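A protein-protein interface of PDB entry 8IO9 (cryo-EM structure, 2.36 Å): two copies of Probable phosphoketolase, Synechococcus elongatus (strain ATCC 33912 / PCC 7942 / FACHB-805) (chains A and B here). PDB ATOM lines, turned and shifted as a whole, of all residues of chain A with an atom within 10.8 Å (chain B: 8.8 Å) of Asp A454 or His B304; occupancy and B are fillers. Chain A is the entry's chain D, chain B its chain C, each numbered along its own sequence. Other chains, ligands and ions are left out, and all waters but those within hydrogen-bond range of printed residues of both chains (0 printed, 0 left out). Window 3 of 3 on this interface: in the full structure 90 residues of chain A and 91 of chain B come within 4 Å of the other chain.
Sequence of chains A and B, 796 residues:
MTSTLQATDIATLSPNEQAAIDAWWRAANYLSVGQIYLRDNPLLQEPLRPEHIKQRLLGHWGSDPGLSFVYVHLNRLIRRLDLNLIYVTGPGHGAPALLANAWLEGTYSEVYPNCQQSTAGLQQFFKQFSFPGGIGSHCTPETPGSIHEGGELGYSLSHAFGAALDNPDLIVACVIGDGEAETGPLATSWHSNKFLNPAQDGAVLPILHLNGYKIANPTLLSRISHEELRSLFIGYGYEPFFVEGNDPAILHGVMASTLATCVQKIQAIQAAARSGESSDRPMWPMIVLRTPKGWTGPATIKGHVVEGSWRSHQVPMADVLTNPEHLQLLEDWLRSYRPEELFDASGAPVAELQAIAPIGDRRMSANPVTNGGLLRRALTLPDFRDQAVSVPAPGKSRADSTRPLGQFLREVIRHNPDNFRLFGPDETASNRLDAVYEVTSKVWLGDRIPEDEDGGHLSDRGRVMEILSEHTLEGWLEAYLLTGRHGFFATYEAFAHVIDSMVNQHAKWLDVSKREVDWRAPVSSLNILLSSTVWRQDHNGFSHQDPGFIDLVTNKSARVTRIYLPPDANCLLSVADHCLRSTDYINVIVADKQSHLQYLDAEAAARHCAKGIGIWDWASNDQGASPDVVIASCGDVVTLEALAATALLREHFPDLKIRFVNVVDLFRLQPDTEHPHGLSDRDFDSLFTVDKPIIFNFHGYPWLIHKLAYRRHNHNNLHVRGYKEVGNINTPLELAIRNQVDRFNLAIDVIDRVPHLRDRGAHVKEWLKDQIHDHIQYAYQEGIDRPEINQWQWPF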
ATOM      1  N   ASP A 434      -1.244  31.837   6.836  1.00  0.00           N
ATOM      2  CA  ASP A 434      -0.576  30.570   7.105  1.00  0.00           C
ATOM      3  C   ASP A 434       0.869  30.731   7.553  1.00  0.00           C
ATOM      4  O   ASP A 434       1.490  29.734   7.935  1.00  0.00           O
ATOM      5  CB  ASP A 434      -0.632  29.674   5.868  1.00  0.00           C
ATOM      6  CG  ASP A 434      -2.007  29.087   5.642  1.00  0.00           C
ATOM      7  OD1 ASP A 434      -2.912  29.383   6.448  1.00  0.00           O
ATOM      8  OD2 ASP A 434      -2.183  28.330   4.664  1.00  0.00           O
ATOM      9  N   TYR A 437       1.711  29.233  10.789  1.00  0.00           N
ATOM     10  CA  TYR A 437       1.877  27.785  10.847  1.00  0.00           C
ATOM     11  C   TYR A 437       3.332  27.355  10.733  1.00  0.00           C
ATOM     12  O   TYR A 437       3.634  26.183  10.980  1.00  0.00           O
ATOM     13  CB  TYR A 437       1.064  27.113   9.743  1.00  0.00           C
ATOM     14  CG  TYR A 437      -0.425  27.291   9.885  1.00  0.00           C
ATOM     15  CD1 TYR A 437      -1.007  27.485  11.129  1.00  0.00           C
ATOM     16  CD2 TYR A 437      -1.252  27.267   8.772  1.00  0.00           C
ATOM     17  CE1 TYR A 437      -2.367  27.650  11.260  1.00  0.00           C
ATOM     18  CE2 TYR A 437      -2.613  27.430   8.894  1.00  0.00           C
ATOM     19  CZ  TYR A 437      -3.164  27.623  10.138  1.00  0.00           C
ATOM     20  OH  TYR A 437      -4.524  27.786  10.258  1.00  0.00           O
ATOM     21  N   THR A 440       4.112  27.510  14.741  1.00  0.00           N
ATOM     22  CA  THR A 440       3.181  26.800  15.607  1.00  0.00           C
ATOM     23  C   THR A 440       2.153  26.044  14.778  1.00  0.00           C
ATOM     24  O   THR A 440       2.292  25.931  13.558  1.00  0.00           O
ATOM     25  CB  THR A 440       2.489  27.769  16.571  1.00  0.00           C
ATOM     26  OG1 THR A 440       1.595  27.041  17.422  1.00  0.00           O
ATOM     27  CG2 THR A 440       1.706  28.822  15.804  1.00  0.00           C
ATOM     28  N   SER A 441       1.126  25.512  15.433  1.00  0.00           N
ATOM     29  CA  SER A 441       0.066  24.787  14.750  1.00  0.00           C
ATOM     30  C   SER A 441      -1.256  25.159  15.409  1.00  0.00           C
ATOM     31  O   SER A 441      -1.339  26.119  16.179  1.00  0.00           O
ATOM     32  CB  SER A 441       0.333  23.277  14.776  1.00  0.00           C
ATOM     33  OG  SER A 441       1.544  22.968  14.110  1.00  0.00           O
ATOM     34  N   LYS A 442      -2.299  24.404  15.092  1.00  0.00           N
ATOM     35  CA  LYS A 442      -3.621  24.632  15.650  1.00  0.00           C
ATOM     36  C   LYS A 442      -3.920  23.599  16.728  1.00  0.00           C
ATOM     37  O   LYS A 442      -3.517  22.439  16.629  1.00  0.00           O
ATOM     38  CB  LYS A 442      -4.686  24.583  14.555  1.00  0.00           C
ATOM     39  CG  LYS A 442      -4.591  25.731  13.570  1.00  0.00           C
ATOM     40  CD  LYS A 442      -5.415  25.477  12.321  1.00  0.00           C
ATOM     41  CE  LYS A 442      -4.824  24.369  11.475  1.00  0.00           C
ATOM     42  NZ  LYS A 442      -5.532  24.236  10.172  1.00  0.00           N
ATOM     43  N   ARG A 448      -6.753  11.744  15.666  1.00  0.00           N
ATOM     44  CA  ARG A 448      -5.786  12.132  14.653  1.00  0.00           C
ATOM     45  C   ARG A 448      -5.637  11.015  13.630  1.00  0.00           C
ATOM     46  O   ARG A 448      -5.711   9.829  13.964  1.00  0.00           O
ATOM     47  CB  ARG A 448      -4.424  12.451  15.278  1.00  0.00           C
ATOM     48  CG  ARG A 448      -4.445  13.628  16.232  1.00  0.00           C
ATOM     49  CD  ARG A 448      -4.631  14.933  15.485  1.00  0.00           C
ATOM     50  NE  ARG A 448      -3.512  15.205  14.593  1.00  0.00           N
ATOM     51  CZ  ARG A 448      -2.397  15.821  14.957  1.00  0.00           C
ATOM     52  NH1 ARG A 448      -2.219  16.254  16.194  1.00  0.00           N
ATOM     53  NH2 ARG A 448      -1.434  16.008  14.059  1.00  0.00           N
ATOM     54  N   ILE A 449      -5.428  11.407  12.378  1.00  0.00           N
ATOM     55  CA  ILE A 449      -5.270  10.453  11.283  1.00  0.00           C
ATOM     56  C   ILE A 449      -4.004  10.813  10.517  1.00  0.00           C
ATOM     57  O   ILE A 449      -3.534  11.960  10.572  1.00  0.00           O
ATOM     58  CB  ILE A 449      -6.506  10.441  10.351  1.00  0.00           C
ATOM     59  CG1 ILE A 449      -6.701  11.807   9.694  1.00  0.00           C
ATOM     60  CG2 ILE A 449      -7.755  10.024  11.115  1.00  0.00           C
ATOM     61  CD1 ILE A 449      -7.800  11.819   8.665  1.00  0.00           C
ATOM     62  N   PRO A 450      -3.411   9.845   9.808  1.00  0.00           N
ATOM     63  CA  PRO A 450      -2.197  10.153   9.035  1.00  0.00           C
ATOM     64  C   PRO A 450      -2.405  11.209   7.963  1.00  0.00           C
ATOM     65  O   PRO A 450      -1.445  11.887   7.582  1.00  0.00           O
ATOM     66  CB  PRO A 450      -1.817   8.796   8.424  1.00  0.00           C
ATOM     67  CG  PRO A 450      -3.077   7.991   8.462  1.00  0.00           C
ATOM     68  CD  PRO A 450      -3.769   8.420   9.713  1.00  0.00           C
ATOM     69  N   GLU A 451      -3.632  11.362   7.459  1.00  0.00           N
ATOM     70  CA  GLU A 451      -3.903  12.391   6.461  1.00  0.00           C
ATOM     71  C   GLU A 451      -3.708  13.796   7.013  1.00  0.00           C
ATOM     72  O   GLU A 451      -3.449  14.723   6.238  1.00  0.00           O
ATOM     73  CB  GLU A 451      -5.327  12.236   5.919  1.00  0.00           C
ATOM     74  CG  GLU A 451      -5.529  11.033   5.007  1.00  0.00           C
ATOM     75  CD  GLU A 451      -5.549   9.713   5.757  1.00  0.00           C
ATOM     76  OE1 GLU A 451      -5.699   9.732   6.996  1.00  0.00           O
ATOM     77  OE2 GLU A 451      -5.412   8.656   5.105  1.00  0.00           O
ATOM     78  N   ASP A 452      -3.818  13.975   8.330  1.00  0.00           N
ATOM     79  CA  ASP A 452      -3.593  15.279   8.940  1.00  0.00           C
ATOM     80  C   ASP A 452      -2.126  15.689   8.939  1.00  0.00           C
ATOM     81  O   ASP A 452      -1.827  16.848   9.239  1.00  0.00           O
ATOM     82  CB  ASP A 452      -4.121  15.290  10.376  1.00  0.00           C
ATOM     83  CG  ASP A 452      -5.621  15.091  10.450  1.00  0.00           C
ATOM     84  OD1 ASP A 452      -6.265  14.987   9.385  1.00  0.00           O
ATOM     85  OD2 ASP A 452      -6.157  15.037  11.576  1.00  0.00           O
ATOM     86  N   GLU A 453      -1.210  14.773   8.622  1.00  0.00           N
ATOM     87  CA  GLU A 453       0.210  15.102   8.672  1.00  0.00           C
ATOM     88  C   GLU A 453       0.618  16.049   7.550  1.00  0.00           C
ATOM     89  O   GLU A 453       1.544  16.848   7.725  1.00  0.00           O
ATOM     90  CB  GLU A 453       1.048  13.825   8.615  1.00  0.00           C
ATOM     91  CG  GLU A 453       0.787  12.857   9.758  1.00  0.00           C
ATOM     92  CD  GLU A 453       1.213  13.409  11.105  1.00  0.00           C
ATOM     93  OE1 GLU A 453       2.099  14.290  11.140  1.00  0.00           O
ATOM     94  OE2 GLU A 453       0.661  12.960  12.131  1.00  0.00           O
ATOM     95  N   ASP A 454      -0.049  15.972   6.397  1.00  0.00           N
ATOM     96  CA  ASP A 454       0.380  16.750   5.238  1.00  0.00           C
ATOM     97  C   ASP A 454       0.183  18.244   5.469  1.00  0.00           C
ATOM     98  O   ASP A 454       1.151  19.012   5.505  1.00  0.00           O
ATOM     99  CB  ASP A 454      -0.381  16.289   3.993  1.00  0.00           C
ATOM    100  CG  ASP A 454       0.191  16.867   2.713  1.00  0.00           C
ATOM    101  OD1 ASP A 454       1.318  17.401   2.750  1.00  0.00           O
ATOM    102  OD2 ASP A 454      -0.490  16.788   1.668  1.00  0.00           O
ATOM    103  N   GLY A 455      -1.062  18.674   5.639  1.00  0.00           N
ATOM    104  CA  GLY A 455      -1.343  20.084   5.815  1.00  0.00           C
ATOM    105  C   GLY A 455      -2.332  20.358   6.925  1.00  0.00           C
ATOM    106  O   GLY A 455      -2.950  21.426   6.967  1.00  0.00           O
ATOM    107  N   GLY A 456      -2.494  19.393   7.832  1.00  0.00           N
ATOM    108  CA  GLY A 456      -3.446  19.561   8.916  1.00  0.00           C
ATOM    109  C   GLY A 456      -3.076  20.691   9.856  1.00  0.00           C
ATOM    110  O   GLY A 456      -3.948  21.431  10.320  1.00  0.00           O
ATOM    111  N   HIS A 457      -1.783  20.845  10.144  1.00  0.00           N
ATOM    112  CA  HIS A 457      -1.286  21.846  11.090  1.00  0.00           C
ATOM    113  C   HIS A 457      -1.962  21.696  12.451  1.00  0.00           C
ATOM    114  O   HIS A 457      -2.382  22.670  13.077  1.00  0.00           O
ATOM    115  CB  HIS A 457      -1.464  23.263  10.543  1.00  0.00           C
ATOM    116  CG  HIS A 457      -0.646  23.548   9.323  1.00  0.00           C
ATOM    117  ND1 HIS A 457       0.722  23.704   9.365  1.00  0.00           N
ATOM    118  CD2 HIS A 457      -1.005  23.713   8.028  1.00  0.00           C
ATOM    119  CE1 HIS A 457       1.173  23.948   8.147  1.00  0.00           C
ATOM    120  NE2 HIS A 457       0.145  23.960   7.317  1.00  0.00           N
ATOM    121  N   LEU A 458      -2.065  20.453  12.907  1.00  0.00           N
ATOM    122  CA  LEU A 458      -2.768  20.122  14.138  1.00  0.00           C
ATOM    123  C   LEU A 458      -1.774  19.610  15.169  1.00  0.00           C
ATOM    124  O   LEU A 458      -1.027  18.665  14.899  1.00  0.00           O
ATOM    125  CB  LEU A 458      -3.849  19.068  13.885  1.00  0.00           C
ATOM    126  CG  LEU A 458      -4.833  19.344  12.748  1.00  0.00           C
ATOM    127  CD1 LEU A 458      -5.762  18.158  12.556  1.00  0.00           C
ATOM    128  CD2 LEU A 458      -5.626  20.612  13.017  1.00  0.00           C
ATOM    129  N   TYR B 213     -14.748  16.975   7.562  1.00  0.00           N
ATOM    130  CA  TYR B 213     -13.921  18.161   7.408  1.00  0.00           C
ATOM    131  C   TYR B 213     -14.778  19.400   7.207  1.00  0.00           C
ATOM    132  O   TYR B 213     -15.883  19.339   6.661  1.00  0.00           O
ATOM    133  CB  TYR B 213     -12.948  18.007   6.235  1.00  0.00           C
ATOM    134  CG  TYR B 213     -11.780  17.096   6.528  1.00  0.00           C
ATOM    135  CD1 TYR B 213     -10.652  17.575   7.175  1.00  0.00           C
ATOM    136  CD2 TYR B 213     -11.803  15.760   6.157  1.00  0.00           C
ATOM    137  CE1 TYR B 213      -9.583  16.753   7.446  1.00  0.00           C
ATOM    138  CE2 TYR B 213     -10.738  14.928   6.426  1.00  0.00           C
ATOM    139  CZ  TYR B 213      -9.631  15.431   7.070  1.00  0.00           C
ATOM    140  OH  TYR B 213      -8.563  14.612   7.341  1.00  0.00           O
ATOM    141  N   PRO B 298     -11.804  14.063  -8.258  1.00  0.00           N
ATOM    142  CA  PRO B 298     -10.390  13.673  -8.326  1.00  0.00           C
ATOM    143  C   PRO B 298      -9.886  13.126  -6.999  1.00  0.00           C
ATOM    144  O   PRO B 298     -10.268  13.593  -5.925  1.00  0.00           O
ATOM    145  CB  PRO B 298      -9.682  14.980  -8.698  1.00  0.00           C
ATOM    146  CG  PRO B 298     -10.737  15.815  -9.336  1.00  0.00           C
ATOM    147  CD  PRO B 298     -12.007  15.471  -8.630  1.00  0.00           C
ATOM    148  N   ALA B 299      -9.011  12.122  -7.086  1.00  0.00           N
ATOM    149  CA  ALA B 299      -8.468  11.496  -5.888  1.00  0.00           C
ATOM    150  C   ALA B 299      -7.351  12.334  -5.276  1.00  0.00           C
ATOM    151  O   ALA B 299      -7.371  12.626  -4.075  1.00  0.00           O
ATOM    152  CB  ALA B 299      -7.965  10.090  -6.214  1.00  0.00           C
ATOM    153  N   THR B 300      -6.364  12.721  -6.083  1.00  0.00           N
ATOM    154  CA  THR B 300      -5.253  13.539  -5.619  1.00  0.00           C
ATOM    155  C   THR B 300      -4.944  14.604  -6.659  1.00  0.00           C
ATOM    156  O   THR B 300      -5.120  14.391  -7.861  1.00  0.00           O
ATOM    157  CB  THR B 300      -3.986  12.709  -5.351  1.00  0.00           C
ATOM    158  OG1 THR B 300      -3.643  11.961  -6.524  1.00  0.00           O
ATOM    159  CG2 THR B 300      -4.192  11.756  -4.184  1.00  0.00           C
ATOM    160  N   ILE B 301      -4.479  15.755  -6.181  1.00  0.00           N
ATOM    161  CA  ILE B 301      -4.070  16.866  -7.031  1.00  0.00           C
ATOM    162  C   ILE B 301      -2.720  17.360  -6.534  1.00  0.00           C
ATOM    163  O   ILE B 301      -2.584  17.711  -5.356  1.00  0.00           O
ATOM    164  CB  ILE B 301      -5.099  18.008  -7.027  1.00  0.00           C
ATOM    165  CG1 ILE B 301      -6.413  17.553  -7.660  1.00  0.00           C
ATOM    166  CG2 ILE B 301      -4.552  19.223  -7.753  1.00  0.00           C
ATOM    167  CD1 ILE B 301      -6.276  17.135  -9.098  1.00  0.00           C
ATOM    168  N   LYS B 302      -1.728  17.384  -7.427  1.00  0.00           N
ATOM    169  CA  LYS B 302      -0.382  17.872  -7.114  1.00  0.00           C
ATOM    170  C   LYS B 302       0.225  17.132  -5.925  1.00  0.00           C
ATOM    171  O   LYS B 302       0.948  17.712  -5.113  1.00  0.00           O
ATOM    172  CB  LYS B 302      -0.385  19.381  -6.862  1.00  0.00           C
ATOM    173  CG  LYS B 302      -0.941  20.203  -8.005  1.00  0.00           C
ATOM    174  CD  LYS B 302      -1.036  21.669  -7.622  1.00  0.00           C
ATOM    175  CE  LYS B 302      -1.717  22.477  -8.711  1.00  0.00           C
ATOM    176  NZ  LYS B 302      -1.891  23.904  -8.324  1.00  0.00           N
ATOM    177  N   GLY B 303      -0.069  15.839  -5.818  1.00  0.00           N
ATOM    178  CA  GLY B 303       0.464  15.031  -4.743  1.00  0.00           C
ATOM    179  C   GLY B 303      -0.245  15.166  -3.414  1.00  0.00           C
ATOM    180  O   GLY B 303       0.206  14.565  -2.429  1.00  0.00           O
ATOM    181  N   HIS B 304      -1.327  15.935  -3.345  1.00  0.00           N
ATOM    182  CA  HIS B 304      -2.109  16.087  -2.127  1.00  0.00           C
ATOM    183  C   HIS B 304      -3.455  15.402  -2.306  1.00  0.00           C
ATOM    184  O   HIS B 304      -4.116  15.585  -3.333  1.00  0.00           O
ATOM    185  CB  HIS B 304      -2.315  17.563  -1.781  1.00  0.00           C
ATOM    186  CG  HIS B 304      -1.044  18.304  -1.513  1.00  0.00           C
ATOM    187  ND1 HIS B 304      -0.245  18.040  -0.421  1.00  0.00           N
ATOM    188  CD2 HIS B 304      -0.437  19.307  -2.189  1.00  0.00           C
ATOM    189  CE1 HIS B 304       0.802  18.846  -0.440  1.00  0.00           C
ATOM    190  NE2 HIS B 304       0.709  19.624  -1.503  1.00  0.00           N
ATOM    191  N   VAL B 305      -3.855  14.612  -1.310  1.00  0.00           N
ATOM    192  CA  VAL B 305      -5.153  13.954  -1.354  1.00  0.00           C
ATOM    193  C   VAL B 305      -6.250  15.008  -1.300  1.00  0.00           C
ATOM    194  O   VAL B 305      -6.201  15.940  -0.488  1.00  0.00           O
ATOM    195  CB  VAL B 305      -5.279  12.940  -0.205  1.00  0.00           C
ATOM    196  CG1 VAL B 305      -4.784  13.541   1.100  1.00  0.00           C
ATOM    197  CG2 VAL B 305      -6.716  12.466  -0.064  1.00  0.00           C
ATOM    198  N   VAL B 306      -7.241  14.874  -2.180  1.00  0.00           N
ATOM    199  CA  VAL B 306      -8.291  15.878  -2.301  1.00  0.00           C
ATOM    200  C   VAL B 306      -9.629  15.280  -1.887  1.00  0.00           C
ATOM    201  O   VAL B 306     -10.296  15.799  -0.984  1.00  0.00           O
ATOM    202  CB  VAL B 306      -8.347  16.443  -3.730  1.00  0.00           C
ATOM    203  CG1 VAL B 306      -9.531  17.365  -3.891  1.00  0.00           C
ATOM    204  CG2 VAL B 306      -7.063  17.184  -4.042  1.00  0.00           C
ATOM    205  N   GLU B 307     -10.028  14.188  -2.536  1.00  0.00           N
ATOM    206  CA  GLU B 307     -11.272  13.521  -2.176  1.00  0.00           C
ATOM    207  C   GLU B 307     -11.198  12.986  -0.751  1.00  0.00           C
ATOM    208  O   GLU B 307     -10.187  12.412  -0.336  1.00  0.00           O
ATOM    209  CB  GLU B 307     -11.568  12.386  -3.154  1.00  0.00           C
ATOM    210  CG  GLU B 307     -12.644  11.429  -2.679  1.00  0.00           C
ATOM    211  CD  GLU B 307     -13.009  10.400  -3.720  1.00  0.00           C
ATOM    212  OE1 GLU B 307     -12.870  10.694  -4.925  1.00  0.00           O
ATOM    213  OE2 GLU B 307     -13.443   9.296  -3.333  1.00  0.00           O
ATOM    214  N   SER B 309     -11.219  14.941   1.876  1.00  0.00           N
ATOM    215  CA  SER B 309     -10.342  15.855   2.588  1.00  0.00           C
ATOM    216  C   SER B 309     -10.867  17.271   2.420  1.00  0.00           C
ATOM    217  O   SER B 309     -11.693  17.549   1.547  1.00  0.00           O
ATOM    218  CB  SER B 309      -8.898  15.759   2.087  1.00  0.00           C
ATOM    219  OG  SER B 309      -8.070  16.694   2.754  1.00  0.00           O
ATOM    220  N   TRP B 310     -10.372  18.168   3.273  1.00  0.00           N
ATOM    221  CA  TRP B 310     -10.796  19.561   3.216  1.00  0.00           C
ATOM    222  C   TRP B 310     -10.360  20.252   1.932  1.00  0.00           C
ATOM    223  O   TRP B 310     -10.895  21.317   1.606  1.00  0.00           O
ATOM    224  CB  TRP B 310     -10.261  20.325   4.427  1.00  0.00           C
ATOM    225  CG  TRP B 310      -8.780  20.212   4.614  1.00  0.00           C
ATOM    226  CD1 TRP B 310      -8.118  19.280   5.355  1.00  0.00           C
ATOM    227  CD2 TRP B 310      -7.777  21.068   4.058  1.00  0.00           C
ATOM    228  NE1 TRP B 310      -6.765  19.499   5.293  1.00  0.00           N
ATOM    229  CE2 TRP B 310      -6.529  20.592   4.502  1.00  0.00           C
ATOM    230  CE3 TRP B 310      -7.812  22.192   3.227  1.00  0.00           C
ATOM    231  CZ2 TRP B 310      -5.329  21.198   4.144  1.00  0.00           C
ATOM    232  CZ3 TRP B 310      -6.619  22.790   2.872  1.00  0.00           C
ATOM    233  CH2 TRP B 310      -5.396  22.293   3.329  1.00  0.00           C
ATOM    234  N   ARG B 311      -9.401  19.679   1.201  1.00  0.00           N
ATOM    235  CA  ARG B 311      -8.953  20.282  -0.050  1.00  0.00           C
ATOM    236  C   ARG B 311     -10.016  20.226  -1.138  1.00  0.00           C
ATOM    237  O   ARG B 311      -9.906  20.955  -2.129  1.00  0.00           O
ATOM    238  CB  ARG B 311      -7.672  19.604  -0.531  1.00  0.00           C
ATOM    239  CG  ARG B 311      -6.408  20.314  -0.085  1.00  0.00           C
ATOM    240  CD  ARG B 311      -5.168  19.555  -0.505  1.00  0.00           C
ATOM    241  NE  ARG B 311      -4.911  18.413   0.362  1.00  0.00           N
ATOM    242  CZ  ARG B 311      -4.104  18.439   1.412  1.00  0.00           C
ATOM    243  NH1 ARG B 311      -3.446  19.534   1.749  1.00  0.00           N
ATOM    244  NH2 ARG B 311      -3.952  17.338   2.142  1.00  0.00           N
ATOM    245  N   SER B 312     -11.038  19.389  -0.977  1.00  0.00           N
ATOM    246  CA  SER B 312     -12.116  19.271  -1.949  1.00  0.00           C
ATOM    247  C   SER B 312     -13.328  20.123  -1.604  1.00  0.00           C
ATOM    248  O   SER B 312     -14.366  19.979  -2.255  1.00  0.00           O
ATOM    249  CB  SER B 312     -12.556  17.814  -2.077  1.00  0.00           C
ATOM    250  OG  SER B 312     -13.169  17.371  -0.881  1.00  0.00           O
ATOM    251  N   PRO B 316     -11.742  21.285  -6.406  1.00  0.00           N
ATOM    252  CA  PRO B 316     -10.510  20.484  -6.326  1.00  0.00           C
ATOM    253  C   PRO B 316      -9.384  21.010  -7.197  1.00  0.00           C
ATOM    254  O   PRO B 316      -8.205  20.824  -6.865  1.00  0.00           O
ATOM    255  CB  PRO B 316     -10.968  19.093  -6.791  1.00  0.00           C
ATOM    256  CG  PRO B 316     -12.443  19.122  -6.755  1.00  0.00           C
ATOM    257  CD  PRO B 316     -12.843  20.529  -7.017  1.00  0.00           C
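OH of Tyr B213 is in hydrogen-bond range of OD1 of Asp A452, 3.1 Å away.
A ring nitrogen (ND1) of His B304 sits at hydrogen-bond distance from the side-chain carboxylate of Asp A454.
OD2 of Asp A454 lies within salt-bridge range of NH2 of Arg B311 (3.5 Å).
The backbone carbonyl oxygen (O) of Val B305 sits at hydrogen-bond distance from the guanidinium group (NE) of Arg B311.
CD1 of Ile A449 touches OH of Tyr B213, at 3.2 Å.
CZ2 of Trp B310 touches O of Gly A455, 3.7 Å away.
Lys A442 touches none of the printed residues of chain B.
Of the printed residues of chain B, Ile A449 touches Tyr B213 (3.2 Å).
Of chain B, only His B304 and Arg B311 come within 4 Å of Asp A454.
Of chain B, only Trp B310 comes within 4 Å of Gly A455.
Thr B300 touches none of the printed residues of chain A.
No residue of chain A comes within 4 Å of Gly B303.
Of chain A, only Asp A454 (2.4 Å) comes within 4 Å of His B304.
No residue of chain A comes within 4 Å of Val B305.
Ser B309 touches none of the printed residues of chain A.
Of the printed residues of chain A, Arg B311 touches Asp A454 (3.5 Å).
The nearest residue of chain B that does not touch Asp A454 is Gly B303 (4.7 Å).
The nearest residue of chain A that does not touch His B304 is Gly A455 (6.1 Å).
Of the 16 printed residues of chain B, 4 touch a printed residue of chain A.
Printed residues of chain B that touch a printed residue of chain A: Tyr B213, His B304, Trp B310 and Arg B311.
Along chain A the printed residues that touch a printed residue of chain B span positions 449 to 455.
Among the printed residues, Asp or Glu carboxylates within 4 Å of a Lys or Arg side-chain nitrogen of the other chain: Asp A454 with Arg B311.
No position is printed for both chains.
Of the 5 pairs that touch across the chains among the printed residues, none has its exchanged pair printed and touching as well.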
